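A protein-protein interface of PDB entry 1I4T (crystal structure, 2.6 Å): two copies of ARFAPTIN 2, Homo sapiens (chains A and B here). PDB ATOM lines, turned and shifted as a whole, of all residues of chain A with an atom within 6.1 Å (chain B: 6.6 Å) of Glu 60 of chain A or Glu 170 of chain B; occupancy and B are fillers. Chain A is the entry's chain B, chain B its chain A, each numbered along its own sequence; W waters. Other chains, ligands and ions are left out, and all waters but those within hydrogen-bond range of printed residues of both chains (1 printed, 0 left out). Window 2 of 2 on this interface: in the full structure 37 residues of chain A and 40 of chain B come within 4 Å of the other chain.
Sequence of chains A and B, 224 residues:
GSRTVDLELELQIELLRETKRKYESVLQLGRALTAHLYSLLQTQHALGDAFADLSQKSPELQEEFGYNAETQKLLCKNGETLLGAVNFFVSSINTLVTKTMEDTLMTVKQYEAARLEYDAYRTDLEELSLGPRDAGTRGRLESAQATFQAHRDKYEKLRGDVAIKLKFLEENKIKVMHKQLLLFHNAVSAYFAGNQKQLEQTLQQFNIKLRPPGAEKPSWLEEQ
Hydrophobic or aromatic side chains of chain B within 4 Å of the printed part of chain A: Tyr 23 and Ile 174. Printed residues of chain A that touch a printed residue of chain B: Glu 60, Leu 61 and Phe 65. Hydrophobic or aromatic side chains of chain A within 4 Å of the printed part of chain B: Leu 61 and Phe 65. Among the printed residues, 6 pairs touch across the chains. Among the printed residues, Asp or Glu carboxylates within 4 Å of a Lys or Arg side-chain nitrogen of the other chain: Glu 60 of chain A with Lys 173 of chain B.
Glu 60 of chain A touches Glu 170 of chain B. Glu 60 of chain A touches Ile 174 of chain B (CB to CD1, 3.4 Å). OH of Tyr 23 of chain B touches CD1 of Leu 61 of chain A (3.99 Å). Ile 174 of chain B touches Leu 61 of chain A (O to CD2, 3.7 Å). Tyr 23 of chain B touches Phe 65 of chain A.
No position is printed for both chains.
Water W1 bridges OH of Tyr 23 of chain B (2.6 Å) and OG of Ser 58 of chain A (2.9 Å).
The side-chain carboxylate (OE1) of Glu 170 of chain B is in salt-bridge range of the side-chain amino group (NZ) of Lys 173 of chain B (2.7 Å).
Printed residues of chain B within 4 Å of Phe 65 of chain A: Tyr 23 (3.7 Å). Of the printed residues of chain A, Lys 173 of chain B touches Glu 60. Printed residues of chain A within 4 Å of Ile 174 of chain B: Glu 60 and Leu 61. Lys 175 of chain B touches none of the printed residues of chain A. The nearest residue of chain B that does not touch Glu 60 of chain A is Tyr 23 of chain B (5.4 Å). The nearest printed residue of chain A that does not touch Glu 170 of chain B is Leu 61 of chain A (7.1 Å). The nearest printed residue of chain A that does not touch Ile 174 of chain B is Glu 64 of chain A (5.9 Å).
OE1 of Glu 60 of chain A lies within salt-bridge range of NZ of Lys 173 of chain B (2.7 Å).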
ATOM      1  N   LYS A  57       9.502  29.612  17.726  1.00  0.00           N
ATOM      2  CA  LYS A  57      10.768  28.995  18.081  1.00  0.00           C
ATOM      3  C   LYS A  57      10.697  27.514  18.444  1.00  0.00           C
ATOM      4  O   LYS A  57      11.735  26.859  18.545  1.00  0.00           O
ATOM      5  CB  LYS A  57      11.391  29.767  19.247  1.00  0.00           C
ATOM      6  CG  LYS A  57      12.604  30.607  18.885  1.00  0.00           C
ATOM      7  CD  LYS A  57      12.356  31.536  17.706  1.00  0.00           C
ATOM      8  CE  LYS A  57      11.582  32.770  18.114  1.00  0.00           C
ATOM      9  NZ  LYS A  57      11.446  33.726  16.975  1.00  0.00           N
ATOM     10  N   SER A  58       9.494  26.978  18.638  1.00  0.00           N
ATOM     11  CA  SER A  58       9.359  25.570  19.012  1.00  0.00           C
ATOM     12  C   SER A  58       8.472  24.745  18.089  1.00  0.00           C
ATOM     13  O   SER A  58       7.300  24.540  18.380  1.00  0.00           O
ATOM     14  CB  SER A  58       8.785  25.439  20.426  1.00  0.00           C
ATOM     15  OG  SER A  58       9.394  26.338  21.324  1.00  0.00           O
ATOM     16  N   PRO A  59       9.017  24.226  16.983  1.00  0.00           N
ATOM     17  CA  PRO A  59       8.133  23.435  16.122  1.00  0.00           C
ATOM     18  C   PRO A  59       7.469  22.221  16.798  1.00  0.00           C
ATOM     19  O   PRO A  59       6.327  21.908  16.465  1.00  0.00           O
ATOM     20  CB  PRO A  59       9.040  23.063  14.944  1.00  0.00           C
ATOM     21  CG  PRO A  59      10.399  23.001  15.564  1.00  0.00           C
ATOM     22  CD  PRO A  59      10.396  24.231  16.463  1.00  0.00           C
ATOM     23  N   GLU A  60       8.150  21.548  17.736  1.00  0.00           N
ATOM     24  CA  GLU A  60       7.552  20.378  18.416  1.00  0.00           C
ATOM     25  C   GLU A  60       6.205  20.712  19.078  1.00  0.00           C
ATOM     26  O   GLU A  60       5.309  19.877  19.145  1.00  0.00           O
ATOM     27  CB  GLU A  60       8.462  19.787  19.521  1.00  0.00           C
ATOM     28  CG  GLU A  60       9.893  20.284  19.597  1.00  0.00           C
ATOM     29  CD  GLU A  60      10.006  21.708  20.098  1.00  0.00           C
ATOM     30  OE1 GLU A  60      10.006  21.924  21.327  1.00  0.00           O
ATOM     31  OE2 GLU A  60      10.089  22.618  19.252  1.00  0.00           O
ATOM     32  N   LEU A  61       6.075  21.930  19.581  1.00  0.00           N
ATOM     33  CA  LEU A  61       4.854  22.359  20.245  1.00  0.00           C
ATOM     34  C   LEU A  61       4.325  23.628  19.603  1.00  0.00           C
ATOM     35  O   LEU A  61       3.962  24.567  20.312  1.00  0.00           O
ATOM     36  CB  LEU A  61       5.152  22.632  21.718  1.00  0.00           C
ATOM     37  CG  LEU A  61       5.497  21.410  22.580  1.00  0.00           C
ATOM     38  CD1 LEU A  61       6.250  21.841  23.813  1.00  0.00           C
ATOM     39  CD2 LEU A  61       4.224  20.685  22.966  1.00  0.00           C
ATOM     40  N   GLN A  62       4.274  23.659  18.272  1.00  0.00           N
ATOM     41  CA  GLN A  62       3.831  24.860  17.565  1.00  0.00           C
ATOM     42  C   GLN A  62       2.357  25.186  17.693  1.00  0.00           C
ATOM     43  O   GLN A  62       1.992  26.353  17.864  1.00  0.00           O
ATOM     44  CB  GLN A  62       4.186  24.784  16.078  1.00  0.00           C
ATOM     45  CG  GLN A  62       3.742  26.029  15.311  1.00  0.00           C
ATOM     46  CD  GLN A  62       3.992  25.947  13.810  1.00  0.00           C
ATOM     47  OE1 GLN A  62       3.186  26.435  13.012  1.00  0.00           O
ATOM     48  NE2 GLN A  62       5.118  25.344  13.417  1.00  0.00           N
ATOM     49  N   GLU A  63       1.508  24.166  17.593  1.00  0.00           N
ATOM     50  CA  GLU A  63       0.062  24.376  17.695  1.00  0.00           C
ATOM     51  C   GLU A  63      -0.347  24.809  19.102  1.00  0.00           C
ATOM     52  O   GLU A  63      -1.035  25.820  19.281  1.00  0.00           O
ATOM     53  CB  GLU A  63      -0.697  23.096  17.330  1.00  0.00           C
ATOM     54  CG  GLU A  63      -0.885  22.835  15.836  1.00  0.00           C
ATOM     55  CD  GLU A  63      -1.823  21.652  15.588  1.00  0.00           C
ATOM     56  OE1 GLU A  63      -1.407  20.497  15.842  1.00  0.00           O
ATOM     57  OE2 GLU A  63      -2.981  21.874  15.160  1.00  0.00           O
ATOM     58  N   GLU A  64       0.084  24.024  20.086  1.00  0.00           N
ATOM     59  CA  GLU A  64      -0.210  24.264  21.484  1.00  0.00           C
ATOM     60  C   GLU A  64       0.161  25.675  21.959  1.00  0.00           C
ATOM     61  O   GLU A  64      -0.632  26.325  22.651  1.00  0.00           O
ATOM     62  CB  GLU A  64       0.497  23.216  22.349  1.00  0.00           C
ATOM     63  CG  GLU A  64       0.110  21.782  22.046  1.00  0.00           C
ATOM     64  CD  GLU A  64       0.895  21.192  20.889  1.00  0.00           C
ATOM     65  OE1 GLU A  64       1.204  21.923  19.935  1.00  0.00           O
ATOM     66  OE2 GLU A  64       1.193  19.985  20.925  1.00  0.00           O
ATOM     67  N   PHE A  65       1.354  26.160  21.611  1.00  0.00           N
ATOM     68  CA  PHE A  65       1.737  27.510  22.028  1.00  0.00           C
ATOM     69  C   PHE A  65       0.967  28.479  21.155  1.00  0.00           C
ATOM     70  O   PHE A  65       0.672  29.601  21.567  1.00  0.00           O
ATOM     71  CB  PHE A  65       3.250  27.767  21.854  1.00  0.00           C
ATOM     72  CG  PHE A  65       4.124  27.152  22.932  1.00  0.00           C
ATOM     73  CD1 PHE A  65       5.016  26.124  22.619  1.00  0.00           C
ATOM     74  CD2 PHE A  65       4.082  27.627  24.240  1.00  0.00           C
ATOM     75  CE1 PHE A  65       5.859  25.578  23.598  1.00  0.00           C
ATOM     76  CE2 PHE A  65       4.919  27.091  25.229  1.00  0.00           C
ATOM     77  CZ  PHE A  65       5.814  26.059  24.903  1.00  0.00           C
ATOM     78  N   THR B  19      15.453  27.795  26.006  1.00  0.00           N
ATOM     79  CA  THR B  19      14.120  27.291  26.332  1.00  0.00           C
ATOM     80  C   THR B  19      13.816  27.434  27.829  1.00  0.00           C
ATOM     81  O   THR B  19      12.716  27.828  28.214  1.00  0.00           O
ATOM     82  CB  THR B  19      13.945  25.784  25.953  1.00  0.00           C
ATOM     83  OG1 THR B  19      14.062  25.604  24.534  1.00  0.00           O
ATOM     84  CG2 THR B  19      12.575  25.306  26.374  1.00  0.00           C
ATOM     85  N   TYR B  23      10.879  29.458  29.467  1.00  0.00           N
ATOM     86  CA  TYR B  23       9.928  28.754  30.304  1.00  0.00           C
ATOM     87  C   TYR B  23       9.856  29.393  31.674  1.00  0.00           C
ATOM     88  O   TYR B  23       8.769  29.574  32.213  1.00  0.00           O
ATOM     89  CB  TYR B  23      10.322  27.290  30.422  1.00  0.00           C
ATOM     90  CG  TYR B  23       9.823  26.443  29.285  1.00  0.00           C
ATOM     91  CD1 TYR B  23       9.587  26.989  28.029  1.00  0.00           C
ATOM     92  CD2 TYR B  23       9.626  25.088  29.452  1.00  0.00           C
ATOM     93  CE1 TYR B  23       9.172  26.200  26.971  1.00  0.00           C
ATOM     94  CE2 TYR B  23       9.213  24.286  28.401  1.00  0.00           C
ATOM     95  CZ  TYR B  23       8.995  24.847  27.169  1.00  0.00           C
ATOM     96  OH  TYR B  23       8.657  24.037  26.122  1.00  0.00           O
ATOM     97  N   LYS B 165      20.811  12.330  27.921  1.00  0.00           N
ATOM     98  CA  LYS B 165      19.894  13.153  28.714  1.00  0.00           C
ATOM     99  C   LYS B 165      19.132  14.188  27.899  1.00  0.00           C
ATOM    100  O   LYS B 165      17.950  14.399  28.123  1.00  0.00           O
ATOM    101  CB  LYS B 165      20.622  13.839  29.868  1.00  0.00           C
ATOM    102  CG  LYS B 165      20.925  12.882  31.008  1.00  0.00           C
ATOM    103  CD  LYS B 165      21.282  13.623  32.258  1.00  0.00           C
ATOM    104  CE  LYS B 165      21.407  12.679  33.426  1.00  0.00           C
ATOM    105  NZ  LYS B 165      21.500  13.472  34.698  1.00  0.00           N
ATOM    106  N   LEU B 166      19.794  14.827  26.949  1.00  0.00           N
ATOM    107  CA  LEU B 166      19.124  15.799  26.105  1.00  0.00           C
ATOM    108  C   LEU B 166      17.996  15.124  25.327  1.00  0.00           C
ATOM    109  O   LEU B 166      16.952  15.723  25.075  1.00  0.00           O
ATOM    110  CB  LEU B 166      20.120  16.414  25.120  1.00  0.00           C
ATOM    111  CG  LEU B 166      21.108  17.401  25.734  1.00  0.00           C
ATOM    112  CD1 LEU B 166      22.224  17.652  24.730  1.00  0.00           C
ATOM    113  CD2 LEU B 166      20.397  18.701  26.122  1.00  0.00           C
ATOM    114  N   LYS B 167      18.211  13.872  24.936  1.00  0.00           N
ATOM    115  CA  LYS B 167      17.199  13.153  24.172  1.00  0.00           C
ATOM    116  C   LYS B 167      15.985  12.795  25.039  1.00  0.00           C
ATOM    117  O   LYS B 167      14.844  13.022  24.636  1.00  0.00           O
ATOM    118  CB  LYS B 167      17.798  11.893  23.544  1.00  0.00           C
ATOM    119  CG  LYS B 167      16.970  11.343  22.393  1.00  0.00           C
ATOM    120  CD  LYS B 167      17.502   9.998  21.927  1.00  0.00           C
ATOM    121  CE  LYS B 167      16.788   9.524  20.664  1.00  0.00           C
ATOM    122  NZ  LYS B 167      17.032  10.425  19.496  1.00  0.00           N
ATOM    123  N   PHE B 168      16.220  12.252  26.228  1.00  0.00           N
ATOM    124  CA  PHE B 168      15.107  11.919  27.098  1.00  0.00           C
ATOM    125  C   PHE B 168      14.391  13.201  27.473  1.00  0.00           C
ATOM    126  O   PHE B 168      13.176  13.301  27.354  1.00  0.00           O
ATOM    127  CB  PHE B 168      15.595  11.183  28.349  1.00  0.00           C
ATOM    128  CG  PHE B 168      15.888   9.718  28.112  1.00  0.00           C
ATOM    129  CD1 PHE B 168      16.718   9.002  28.982  1.00  0.00           C
ATOM    130  CD2 PHE B 168      15.314   9.044  27.021  1.00  0.00           C
ATOM    131  CE1 PHE B 168      16.971   7.641  28.771  1.00  0.00           C
ATOM    132  CE2 PHE B 168      15.560   7.685  26.801  1.00  0.00           C
ATOM    133  CZ  PHE B 168      16.388   6.984  27.675  1.00  0.00           C
ATOM    134  N   LEU B 169      15.157  14.197  27.899  1.00  0.00           N
ATOM    135  CA  LEU B 169      14.598  15.477  28.286  1.00  0.00           C
ATOM    136  C   LEU B 169      13.661  16.081  27.246  1.00  0.00           C
ATOM    137  O   LEU B 169      12.592  16.568  27.589  1.00  0.00           O
ATOM    138  CB  LEU B 169      15.727  16.462  28.578  1.00  0.00           C
ATOM    139  CG  LEU B 169      15.267  17.905  28.799  1.00  0.00           C
ATOM    140  CD1 LEU B 169      14.201  17.970  29.902  1.00  0.00           C
ATOM    141  CD2 LEU B 169      16.474  18.759  29.145  1.00  0.00           C
ATOM    142  N   GLU B 170      14.069  16.056  25.983  1.00  0.00           N
ATOM    143  CA  GLU B 170      13.260  16.631  24.924  1.00  0.00           C
ATOM    144  C   GLU B 170      11.950  15.870  24.738  1.00  0.00           C
ATOM    145  O   GLU B 170      10.909  16.474  24.486  1.00  0.00           O
ATOM    146  CB  GLU B 170      14.055  16.663  23.616  1.00  0.00           C
ATOM    147  CG  GLU B 170      13.247  17.097  22.380  1.00  0.00           C
ATOM    148  CD  GLU B 170      12.887  18.579  22.356  1.00  0.00           C
ATOM    149  OE1 GLU B 170      13.242  19.325  23.298  1.00  0.00           O
ATOM    150  OE2 GLU B 170      12.244  18.997  21.371  1.00  0.00           O
ATOM    151  N   GLU B 171      12.015  14.547  24.853  1.00  0.00           N
ATOM    152  CA  GLU B 171      10.844  13.688  24.719  1.00  0.00           C
ATOM    153  C   GLU B 171       9.836  13.998  25.822  1.00  0.00           C
ATOM    154  O   GLU B 171       8.623  14.092  25.579  1.00  0.00           O
ATOM    155  CB  GLU B 171      11.258  12.215  24.807  1.00  0.00           C
ATOM    156  CG  GLU B 171      11.874  11.653  23.543  1.00  0.00           C
ATOM    157  CD  GLU B 171      12.614  10.342  23.782  1.00  0.00           C
ATOM    158  OE1 GLU B 171      12.129   9.504  24.575  1.00  0.00           O
ATOM    159  OE2 GLU B 171      13.684  10.139  23.173  1.00  0.00           O
ATOM    160  N   ASN B 172      10.351  14.162  27.036  1.00  0.00           N
ATOM    161  CA  ASN B 172       9.512  14.460  28.175  1.00  0.00           C
ATOM    162  C   ASN B 172       8.950  15.893  28.137  1.00  0.00           C
ATOM    163  O   ASN B 172       7.829  16.146  28.576  1.00  0.00           O
ATOM    164  CB  ASN B 172      10.313  14.238  29.448  1.00  0.00           C
ATOM    165  CG  ASN B 172       9.576  13.384  30.448  1.00  0.00           C
ATOM    166  OD1 ASN B 172       8.645  13.844  31.116  1.00  0.00           O
ATOM    167  ND2 ASN B 172       9.976  12.118  30.550  1.00  0.00           N
ATOM    168  N   LYS B 173       9.734  16.823  27.602  1.00  0.00           N
ATOM    169  CA  LYS B 173       9.339  18.223  27.512  1.00  0.00           C
ATOM    170  C   LYS B 173       8.102  18.336  26.638  1.00  0.00           C
ATOM    171  O   LYS B 173       7.152  19.041  26.966  1.00  0.00           O
ATOM    172  CB  LYS B 173      10.477  19.054  26.905  1.00  0.00           C
ATOM    173  CG  LYS B 173      10.223  20.550  26.886  1.00  0.00           C
ATOM    174  CD  LYS B 173      11.107  21.256  25.866  1.00  0.00           C
ATOM    175  CE  LYS B 173      10.640  20.951  24.464  1.00  0.00           C
ATOM    176  NZ  LYS B 173      11.579  21.427  23.403  1.00  0.00           N
ATOM    177  N   ILE B 174       8.121  17.631  25.519  1.00  0.00           N
ATOM    178  CA  ILE B 174       6.990  17.638  24.605  1.00  0.00           C
ATOM    179  C   ILE B 174       5.701  17.073  25.241  1.00  0.00           C
ATOM    180  O   ILE B 174       4.636  17.676  25.105  1.00  0.00           O
ATOM    181  CB  ILE B 174       7.352  16.862  23.316  1.00  0.00           C
ATOM    182  CG1 ILE B 174       8.551  17.553  22.637  1.00  0.00           C
ATOM    183  CG2 ILE B 174       6.166  16.808  22.381  1.00  0.00           C
ATOM    184  CD1 ILE B 174       9.008  16.948  21.309  1.00  0.00           C
ATOM    185  N   LYS B 175       5.784  15.943  25.945  1.00  0.00           N
ATOM    186  CA  LYS B 175       4.597  15.346  26.580  1.00  0.00           C
ATOM    187  C   LYS B 175       3.992  16.234  27.654  1.00  0.00           C
ATOM    188  O   LYS B 175       2.781  16.484  27.656  1.00  0.00           O
ATOM    189  CB  LYS B 175       4.929  13.996  27.218  1.00  0.00           C
ATOM    190  CG  LYS B 175       5.256  12.892  26.239  1.00  0.00           C
ATOM    191  CD  LYS B 175       5.901  11.742  26.976  1.00  0.00           C
ATOM    192  CE  LYS B 175       6.512  10.718  26.021  1.00  0.00           C
ATOM    193  NZ  LYS B 175       7.469   9.812  26.764  1.00  0.00           N
HETATM  194  O   HOH W   1       9.509  24.821  23.809  1.00  0.00           O
